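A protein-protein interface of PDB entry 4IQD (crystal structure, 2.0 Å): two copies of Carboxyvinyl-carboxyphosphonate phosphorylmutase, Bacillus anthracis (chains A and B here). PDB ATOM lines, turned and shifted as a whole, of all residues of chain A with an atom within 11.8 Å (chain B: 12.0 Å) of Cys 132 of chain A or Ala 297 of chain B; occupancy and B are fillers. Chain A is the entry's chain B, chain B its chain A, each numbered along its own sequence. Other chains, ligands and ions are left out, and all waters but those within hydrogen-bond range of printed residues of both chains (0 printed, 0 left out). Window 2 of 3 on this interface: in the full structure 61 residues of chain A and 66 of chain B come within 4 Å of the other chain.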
ATOM      1  N   LEU A  69      30.095  -4.528 -17.500  1.00  0.00           N
ATOM      2  CA  LEU A  69      29.297  -3.595 -18.277  1.00  0.00           C
ATOM      3  C   LEU A  69      29.297  -3.952 -19.757  1.00  0.00           C
ATOM      4  O   LEU A  69      28.824  -3.178 -20.589  1.00  0.00           O
ATOM      5  CB  LEU A  69      29.806  -2.170 -18.065  1.00  0.00           C
ATOM      6  CG  LEU A  69      29.582  -1.643 -16.646  1.00  0.00           C
ATOM      7  CD1 LEU A  69      30.248  -0.295 -16.447  1.00  0.00           C
ATOM      8  CD2 LEU A  69      28.091  -1.557 -16.350  1.00  0.00           C
ATOM      9  N   GLN A 127      19.273  -6.430 -22.485  1.00  0.00           N
ATOM     10  CA  GLN A 127      19.633  -5.699 -23.690  1.00  0.00           C
ATOM     11  C   GLN A 127      20.977  -5.005 -23.529  1.00  0.00           C
ATOM     12  O   GLN A 127      21.238  -4.372 -22.508  1.00  0.00           O
ATOM     13  CB  GLN A 127      18.558  -4.682 -24.065  1.00  0.00           C
ATOM     14  CG  GLN A 127      18.660  -4.219 -25.504  1.00  0.00           C
ATOM     15  CD  GLN A 127      18.204  -2.792 -25.690  1.00  0.00           C
ATOM     16  OE1 GLN A 127      17.070  -2.442 -25.368  1.00  0.00           O
ATOM     17  NE2 GLN A 127      19.096  -1.953 -26.205  1.00  0.00           N
ATOM     18  N   LEU A 128      21.827  -5.143 -24.541  1.00  0.00           N
ATOM     19  CA  LEU A 128      23.140  -4.505 -24.550  1.00  0.00           C
ATOM     20  C   LEU A 128      23.483  -3.973 -25.939  1.00  0.00           C
ATOM     21  O   LEU A 128      23.179  -4.617 -26.945  1.00  0.00           O
ATOM     22  CB  LEU A 128      24.219  -5.479 -24.072  1.00  0.00           C
ATOM     23  CG  LEU A 128      24.399  -5.593 -22.557  1.00  0.00           C
ATOM     24  CD1 LEU A 128      25.394  -6.689 -22.212  1.00  0.00           C
ATOM     25  CD2 LEU A 128      24.843  -4.259 -21.969  1.00  0.00           C
ATOM     26  N   PRO A 129      24.121  -2.790 -26.003  1.00  0.00           N
ATOM     27  CA  PRO A 129      24.531  -1.957 -24.864  1.00  0.00           C
ATOM     28  C   PRO A 129      23.363  -1.198 -24.238  1.00  0.00           C
ATOM     29  O   PRO A 129      22.243  -1.257 -24.744  1.00  0.00           O
ATOM     30  CB  PRO A 129      25.512  -0.955 -25.496  1.00  0.00           C
ATOM     31  CG  PRO A 129      25.795  -1.471 -26.874  1.00  0.00           C
ATOM     32  CD  PRO A 129      24.579  -2.222 -27.278  1.00  0.00           C
ATOM     33  N   LYS A 130      23.630  -0.494 -23.143  1.00  0.00           N
ATOM     34  CA  LYS A 130      22.601   0.297 -22.481  1.00  0.00           C
ATOM     35  C   LYS A 130      22.728   1.777 -22.827  1.00  0.00           C
ATOM     36  O   LYS A 130      23.827   2.287 -23.041  1.00  0.00           O
ATOM     37  CB  LYS A 130      22.654   0.090 -20.967  1.00  0.00           C
ATOM     38  CG  LYS A 130      22.181  -1.282 -20.523  1.00  0.00           C
ATOM     39  CD  LYS A 130      22.501  -1.518 -19.065  1.00  0.00           C
ATOM     40  CE  LYS A 130      21.875  -2.799 -18.548  1.00  0.00           C
ATOM     41  NZ  LYS A 130      22.248  -3.035 -17.127  1.00  0.00           N
ATOM     42  N   LYS A 131      21.589   2.457 -22.879  1.00  0.00           N
ATOM     43  CA  LYS A 131      21.532   3.841 -23.327  1.00  0.00           C
ATOM     44  C   LYS A 131      22.199   4.791 -22.342  1.00  0.00           C
ATOM     45  O   LYS A 131      22.422   4.444 -21.181  1.00  0.00           O
ATOM     46  CB  LYS A 131      20.075   4.252 -23.539  1.00  0.00           C
ATOM     47  CG  LYS A 131      19.262   3.211 -24.287  1.00  0.00           C
ATOM     48  CD  LYS A 131      17.910   2.963 -23.630  1.00  0.00           C
ATOM     49  CE  LYS A 131      16.865   3.962 -24.101  1.00  0.00           C
ATOM     50  NZ  LYS A 131      15.522   3.672 -23.521  1.00  0.00           N
ATOM     51  N   CYS A 132      22.525   5.987 -22.818  1.00  0.00           N
ATOM     52  CA  CYS A 132      23.002   7.047 -21.945  1.00  0.00           C
ATOM     53  C   CYS A 132      21.879   7.464 -21.015  1.00  0.00           C
ATOM     54  O   CYS A 132      20.720   7.516 -21.419  1.00  0.00           O
ATOM     55  CB  CYS A 132      23.457   8.252 -22.761  1.00  0.00           C
ATOM     56  SG  CYS A 132      25.130   8.146 -23.390  1.00  0.00           S
ATOM     57  N   GLY A 133      22.226   7.755 -19.766  1.00  0.00           N
ATOM     58  CA  GLY A 133      21.244   8.137 -18.769  1.00  0.00           C
ATOM     59  C   GLY A 133      20.515   6.937 -18.193  1.00  0.00           C
ATOM     60  O   GLY A 133      20.067   6.959 -17.047  1.00  0.00           O
ATOM     61  N   HIS A 134      20.402   5.886 -18.997  1.00  0.00           N
ATOM     62  CA  HIS A 134      19.725   4.667 -18.587  1.00  0.00           C
ATOM     63  C   HIS A 134      20.738   3.548 -18.419  1.00  0.00           C
ATOM     64  O   HIS A 134      20.489   2.403 -18.796  1.00  0.00           O
ATOM     65  CB  HIS A 134      18.673   4.280 -19.623  1.00  0.00           C
ATOM     66  CG  HIS A 134      17.775   5.412 -20.018  1.00  0.00           C
ATOM     67  ND1 HIS A 134      17.220   5.522 -21.273  1.00  0.00           N
ATOM     68  CD2 HIS A 134      17.339   6.490 -19.320  1.00  0.00           C
ATOM     69  CE1 HIS A 134      16.481   6.614 -21.335  1.00  0.00           C
ATOM     70  NE2 HIS A 134      16.536   7.221 -20.162  1.00  0.00           N
ATOM     71  N   LEU A 135      21.892   3.897 -17.860  1.00  0.00           N
ATOM     72  CA  LEU A 135      22.928   2.916 -17.584  1.00  0.00           C
ATOM     73  C   LEU A 135      22.397   1.847 -16.639  1.00  0.00           C
ATOM     74  O   LEU A 135      22.566   0.656 -16.883  1.00  0.00           O
ATOM     75  CB  LEU A 135      24.152   3.589 -16.967  1.00  0.00           C
ATOM     76  CG  LEU A 135      25.354   2.674 -16.743  1.00  0.00           C
ATOM     77  CD1 LEU A 135      26.218   2.623 -17.991  1.00  0.00           C
ATOM     78  CD2 LEU A 135      26.159   3.116 -15.537  1.00  0.00           C
ATOM     79  N   ASN A 136      21.744   2.272 -15.564  1.00  0.00           N
ATOM     80  CA  ASN A 136      21.188   1.330 -14.599  1.00  0.00           C
ATOM     81  C   ASN A 136      19.863   0.726 -15.056  1.00  0.00           C
ATOM     82  O   ASN A 136      19.173   0.067 -14.276  1.00  0.00           O
ATOM     83  CB  ASN A 136      21.022   1.988 -13.229  1.00  0.00           C
ATOM     84  CG  ASN A 136      22.347   2.260 -12.548  1.00  0.00           C
ATOM     85  OD1 ASN A 136      23.363   1.637 -12.867  1.00  0.00           O
ATOM     86  ND2 ASN A 136      22.345   3.189 -11.597  1.00  0.00           N
ATOM     87  N   GLY A 137      19.516   0.954 -16.320  1.00  0.00           N
ATOM     88  CA  GLY A 137      18.279   0.445 -16.888  1.00  0.00           C
ATOM     89  C   GLY A 137      18.207  -1.069 -16.869  1.00  0.00           C
ATOM     90  O   GLY A 137      19.232  -1.749 -16.860  1.00  0.00           O
ATOM     91  N   LYS A 138      16.990  -1.603 -16.867  1.00  0.00           N
ATOM     92  CA  LYS A 138      16.794  -3.040 -16.732  1.00  0.00           C
ATOM     93  C   LYS A 138      15.782  -3.591 -17.725  1.00  0.00           C
ATOM     94  O   LYS A 138      14.916  -4.378 -17.357  1.00  0.00           O
ATOM     95  CB  LYS A 138      16.341  -3.375 -15.311  1.00  0.00           C
ATOM     96  CG  LYS A 138      17.365  -3.060 -14.233  1.00  0.00           C
ATOM     97  CD  LYS A 138      16.704  -3.022 -12.865  1.00  0.00           C
ATOM     98  CE  LYS A 138      15.917  -4.295 -12.602  1.00  0.00           C
ATOM     99  NZ  LYS A 138      14.977  -4.146 -11.456  1.00  0.00           N
ATOM    100  N   ASP B 288      32.574   5.773 -11.144  1.00  0.00           N
ATOM    101  CA  ASP B 288      33.203   6.715 -12.060  1.00  0.00           C
ATOM    102  C   ASP B 288      32.800   6.484 -13.514  1.00  0.00           C
ATOM    103  O   ASP B 288      32.906   7.384 -14.349  1.00  0.00           O
ATOM    104  CB  ASP B 288      34.721   6.677 -11.897  1.00  0.00           C
ATOM    105  CG  ASP B 288      35.158   7.081 -10.502  1.00  0.00           C
ATOM    106  OD1 ASP B 288      35.122   6.222  -9.594  1.00  0.00           O
ATOM    107  OD2 ASP B 288      35.523   8.258 -10.310  1.00  0.00           O
ATOM    108  N   PHE B 289      32.332   5.280 -13.812  1.00  0.00           N
ATOM    109  CA  PHE B 289      31.804   4.991 -15.135  1.00  0.00           C
ATOM    110  C   PHE B 289      30.406   5.568 -15.265  1.00  0.00           C
ATOM    111  O   PHE B 289      30.025   6.075 -16.320  1.00  0.00           O
ATOM    112  CB  PHE B 289      31.775   3.485 -15.381  1.00  0.00           C
ATOM    113  CG  PHE B 289      33.135   2.875 -15.527  1.00  0.00           C
ATOM    114  CD1 PHE B 289      33.763   2.844 -16.759  1.00  0.00           C
ATOM    115  CD2 PHE B 289      33.793   2.342 -14.432  1.00  0.00           C
ATOM    116  CE1 PHE B 289      35.019   2.290 -16.900  1.00  0.00           C
ATOM    117  CE2 PHE B 289      35.051   1.788 -14.568  1.00  0.00           C
ATOM    118  CZ  PHE B 289      35.663   1.759 -15.804  1.00  0.00           C
ATOM    119  N   GLU B 290      29.643   5.484 -14.182  1.00  0.00           N
ATOM    120  CA  GLU B 290      28.288   6.010 -14.159  1.00  0.00           C
ATOM    121  C   GLU B 290      28.299   7.510 -14.409  1.00  0.00           C
ATOM    122  O   GLU B 290      27.535   8.011 -15.230  1.00  0.00           O
ATOM    123  CB  GLU B 290      27.621   5.713 -12.816  1.00  0.00           C
ATOM    124  CG  GLU B 290      27.605   4.242 -12.439  1.00  0.00           C
ATOM    125  CD  GLU B 290      27.024   4.000 -11.057  1.00  0.00           C
ATOM    126  OE1 GLU B 290      27.553   4.565 -10.077  1.00  0.00           O
ATOM    127  OE2 GLU B 290      26.032   3.247 -10.952  1.00  0.00           O
ATOM    128  N   GLU B 291      29.177   8.222 -13.708  1.00  0.00           N
ATOM    129  CA  GLU B 291      29.255   9.671 -13.857  1.00  0.00           C
ATOM    130  C   GLU B 291      29.764  10.039 -15.243  1.00  0.00           C
ATOM    131  O   GLU B 291      29.567  11.157 -15.715  1.00  0.00           O
ATOM    132  CB  GLU B 291      30.134  10.303 -12.771  1.00  0.00           C
ATOM    133  CG  GLU B 291      31.629  10.101 -12.952  1.00  0.00           C
ATOM    134  CD  GLU B 291      32.450  11.100 -12.150  1.00  0.00           C
ATOM    135  OE1 GLU B 291      33.568  10.748 -11.717  1.00  0.00           O
ATOM    136  OE2 GLU B 291      31.977  12.242 -11.958  1.00  0.00           O
ATOM    137  N   LEU B 292      30.415   9.085 -15.895  1.00  0.00           N
ATOM    138  CA  LEU B 292      30.869   9.280 -17.259  1.00  0.00           C
ATOM    139  C   LEU B 292      29.681   9.228 -18.210  1.00  0.00           C
ATOM    140  O   LEU B 292      29.469  10.145 -19.005  1.00  0.00           O
ATOM    141  CB  LEU B 292      31.893   8.212 -17.629  1.00  0.00           C
ATOM    142  CG  LEU B 292      32.625   8.397 -18.956  1.00  0.00           C
ATOM    143  CD1 LEU B 292      33.383   9.713 -18.962  1.00  0.00           C
ATOM    144  CD2 LEU B 292      33.567   7.233 -19.201  1.00  0.00           C
ATOM    145  N   ASP B 293      28.899   8.155 -18.111  1.00  0.00           N
ATOM    146  CA  ASP B 293      27.760   7.935 -19.001  1.00  0.00           C
ATOM    147  C   ASP B 293      26.684   9.015 -18.890  1.00  0.00           C
ATOM    148  O   ASP B 293      26.018   9.340 -19.874  1.00  0.00           O
ATOM    149  CB  ASP B 293      27.137   6.561 -18.741  1.00  0.00           C
ATOM    150  CG  ASP B 293      26.098   6.186 -19.781  1.00  0.00           C
ATOM    151  OD1 ASP B 293      26.360   6.394 -20.983  1.00  0.00           O
ATOM    152  OD2 ASP B 293      25.019   5.690 -19.397  1.00  0.00           O
ATOM    153  N   THR B 294      26.509   9.563 -17.693  1.00  0.00           N
ATOM    154  CA  THR B 294      25.471  10.563 -17.471  1.00  0.00           C
ATOM    155  C   THR B 294      25.964  11.954 -17.844  1.00  0.00           C
ATOM    156  O   THR B 294      25.187  12.797 -18.287  1.00  0.00           O
ATOM    157  CB  THR B 294      24.986  10.570 -16.012  1.00  0.00           C
ATOM    158  OG1 THR B 294      24.881   9.223 -15.536  1.00  0.00           O
ATOM    159  CG2 THR B 294      23.626  11.249 -15.908  1.00  0.00           C
ATOM    160  N   GLY B 295      27.257  12.190 -17.661  1.00  0.00           N
ATOM    161  CA  GLY B 295      27.858  13.445 -18.073  1.00  0.00           C
ATOM    162  C   GLY B 295      27.747  13.625 -19.574  1.00  0.00           C
ATOM    163  O   GLY B 295      27.485  14.725 -20.061  1.00  0.00           O
ATOM    164  N   ILE B 296      27.943  12.533 -20.306  1.00  0.00           N
ATOM    165  CA  ILE B 296      27.806  12.530 -21.756  1.00  0.00           C
ATOM    166  C   ILE B 296      26.339  12.679 -22.150  1.00  0.00           C
ATOM    167  O   ILE B 296      26.010  13.370 -23.116  1.00  0.00           O
ATOM    168  CB  ILE B 296      28.362  11.224 -22.367  1.00  0.00           C
ATOM    169  CG1 ILE B 296      29.852  11.069 -22.055  1.00  0.00           C
ATOM    170  CG2 ILE B 296      28.138  11.194 -23.863  1.00  0.00           C
ATOM    171  CD1 ILE B 296      30.734  12.100 -22.717  1.00  0.00           C
ATOM    172  N   ALA B 297      25.466  12.036 -21.378  1.00  0.00           N
ATOM    173  CA  ALA B 297      24.031  12.000 -21.657  1.00  0.00           C
ATOM    174  C   ALA B 297      23.383  13.384 -21.672  1.00  0.00           C
ATOM    175  O   ALA B 297      22.390  13.604 -22.366  1.00  0.00           O
ATOM    176  CB  ALA B 297      23.327  11.106 -20.649  1.00  0.00           C
ATOM    177  N   LYS B 298      23.950  14.308 -20.902  1.00  0.00           N
ATOM    178  CA  LYS B 298      23.382  15.643 -20.752  1.00  0.00           C
ATOM    179  C   LYS B 298      24.392  16.728 -21.108  1.00  0.00           C
ATOM    180  O   LYS B 298      24.049  17.720 -21.753  1.00  0.00           O
ATOM    181  CB  LYS B 298      22.891  15.836 -19.318  1.00  0.00           C
ATOM    182  CG  LYS B 298      21.929  14.754 -18.856  1.00  0.00           C
ATOM    183  CD  LYS B 298      22.235  14.302 -17.439  1.00  0.00           C
ATOM    184  CE  LYS B 298      22.010  15.420 -16.437  1.00  0.00           C
ATOM    185  NZ  LYS B 298      22.201  14.950 -15.035  1.00  0.00           N
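No position is printed for both chains. Of the 8 pairs that touch across the chains among the printed residues, none has its exchanged pair printed and touching as well.
Of chain B, only Asp 293 and Ala 297 come within 4 Å of Cys 132 of chain A. Ala 297 of chain B touches just these residues of chain A: Cys 132 (3.6 Å) and Gly 133 (3.6 Å). Lys 131 of chain A touches just one residue of chain B: Asp 293. No residue of chain B comes within 4 Å of His 134 of chain A. Asp 293 of chain B touches just these residues of chain A: Lys 131 (3.4 Å), Cys 132 (3.2 Å), Gly 133 (3.5 Å) and Leu 135 (3.3 Å). No residue of chain A comes within 4 Å of Thr 294 of chain B. Gly 295 of chain B touches none of the printed residues of chain A. No residue of chain A comes within 4 Å of Ile 296 of chain B. No residue of chain A comes within 4 Å of Lys 298 of chain B. Of the printed residues of chain A, Glu 290 of chain B touches Leu 135 and Asn 136. Printed residues of chain B within 4 Å of Asn 136 of chain A: Glu 290 (3.7 Å). Of the printed residues of chain B, Leu 135 of chain A touches Glu 290 (3.6 Å) and Asp 293 (3.3 Å). Glu 291 of chain B touches none of the printed residues of chain A. Leu 292 of chain B touches none of the printed residues of chain A. The nearest residue of chain A that does not touch Ala 297 of chain B is His 134 of chain A (6.2 Å). The nearest printed residue of chain B that does not touch Leu 135 of chain A is Phe 289 of chain B (4.9 Å).
Hydrophobic or aromatic side chains of chain A within 4 Å of the printed part of chain B: Leu 135. Of the 11 printed residues of chain B, 3 touch a printed residue of chain A. Hydrophobic or aromatic side chains of chain B that line the printed part of chain A: Ala 297. Among the printed residues, 8 pairs touch across the chains. Among the printed residues, no Asp or Glu carboxylate lies within 4 Å of a Lys or Arg side-chain nitrogen of the other chain.
Among the printed residues, merely in contact across the chains: Leu 135 of chain A with Asp 293 of chain B (3.3 Å), Cys 132 of chain A with Ala 297 of chain B (3.6 Å), Leu 135 of chain A with Glu 290 of chain B (3.6 Å), Gly 133 of chain A with Ala 297 of chain B (3.6 Å) and Asn 136 of chain A with Glu 290 of chain B (3.7 Å).
OG1 of Thr 294 of chain B is in hydrogen-bond range of O of Glu 290 of chain B, 2.9 Å away. The side-chain amino group (NZ) of Lys 131 of chain A sits close to a ring nitrogen (ND1) of His 134 of chain A (3.4 Å).
OD1 of Asp 293 of chain B sits at hydrogen-bond distance from SG of Cys 132 of chain A, 3.2 Å away. The side-chain carboxylate of Asp 293 of chain B is in hydrogen-bond range of the backbone NH of Gly 133 of chain A, at 3.5 Å. O of Lys 131 of chain A lies close to OD2 of Asp 293 of chain B, at 3.4 Å.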
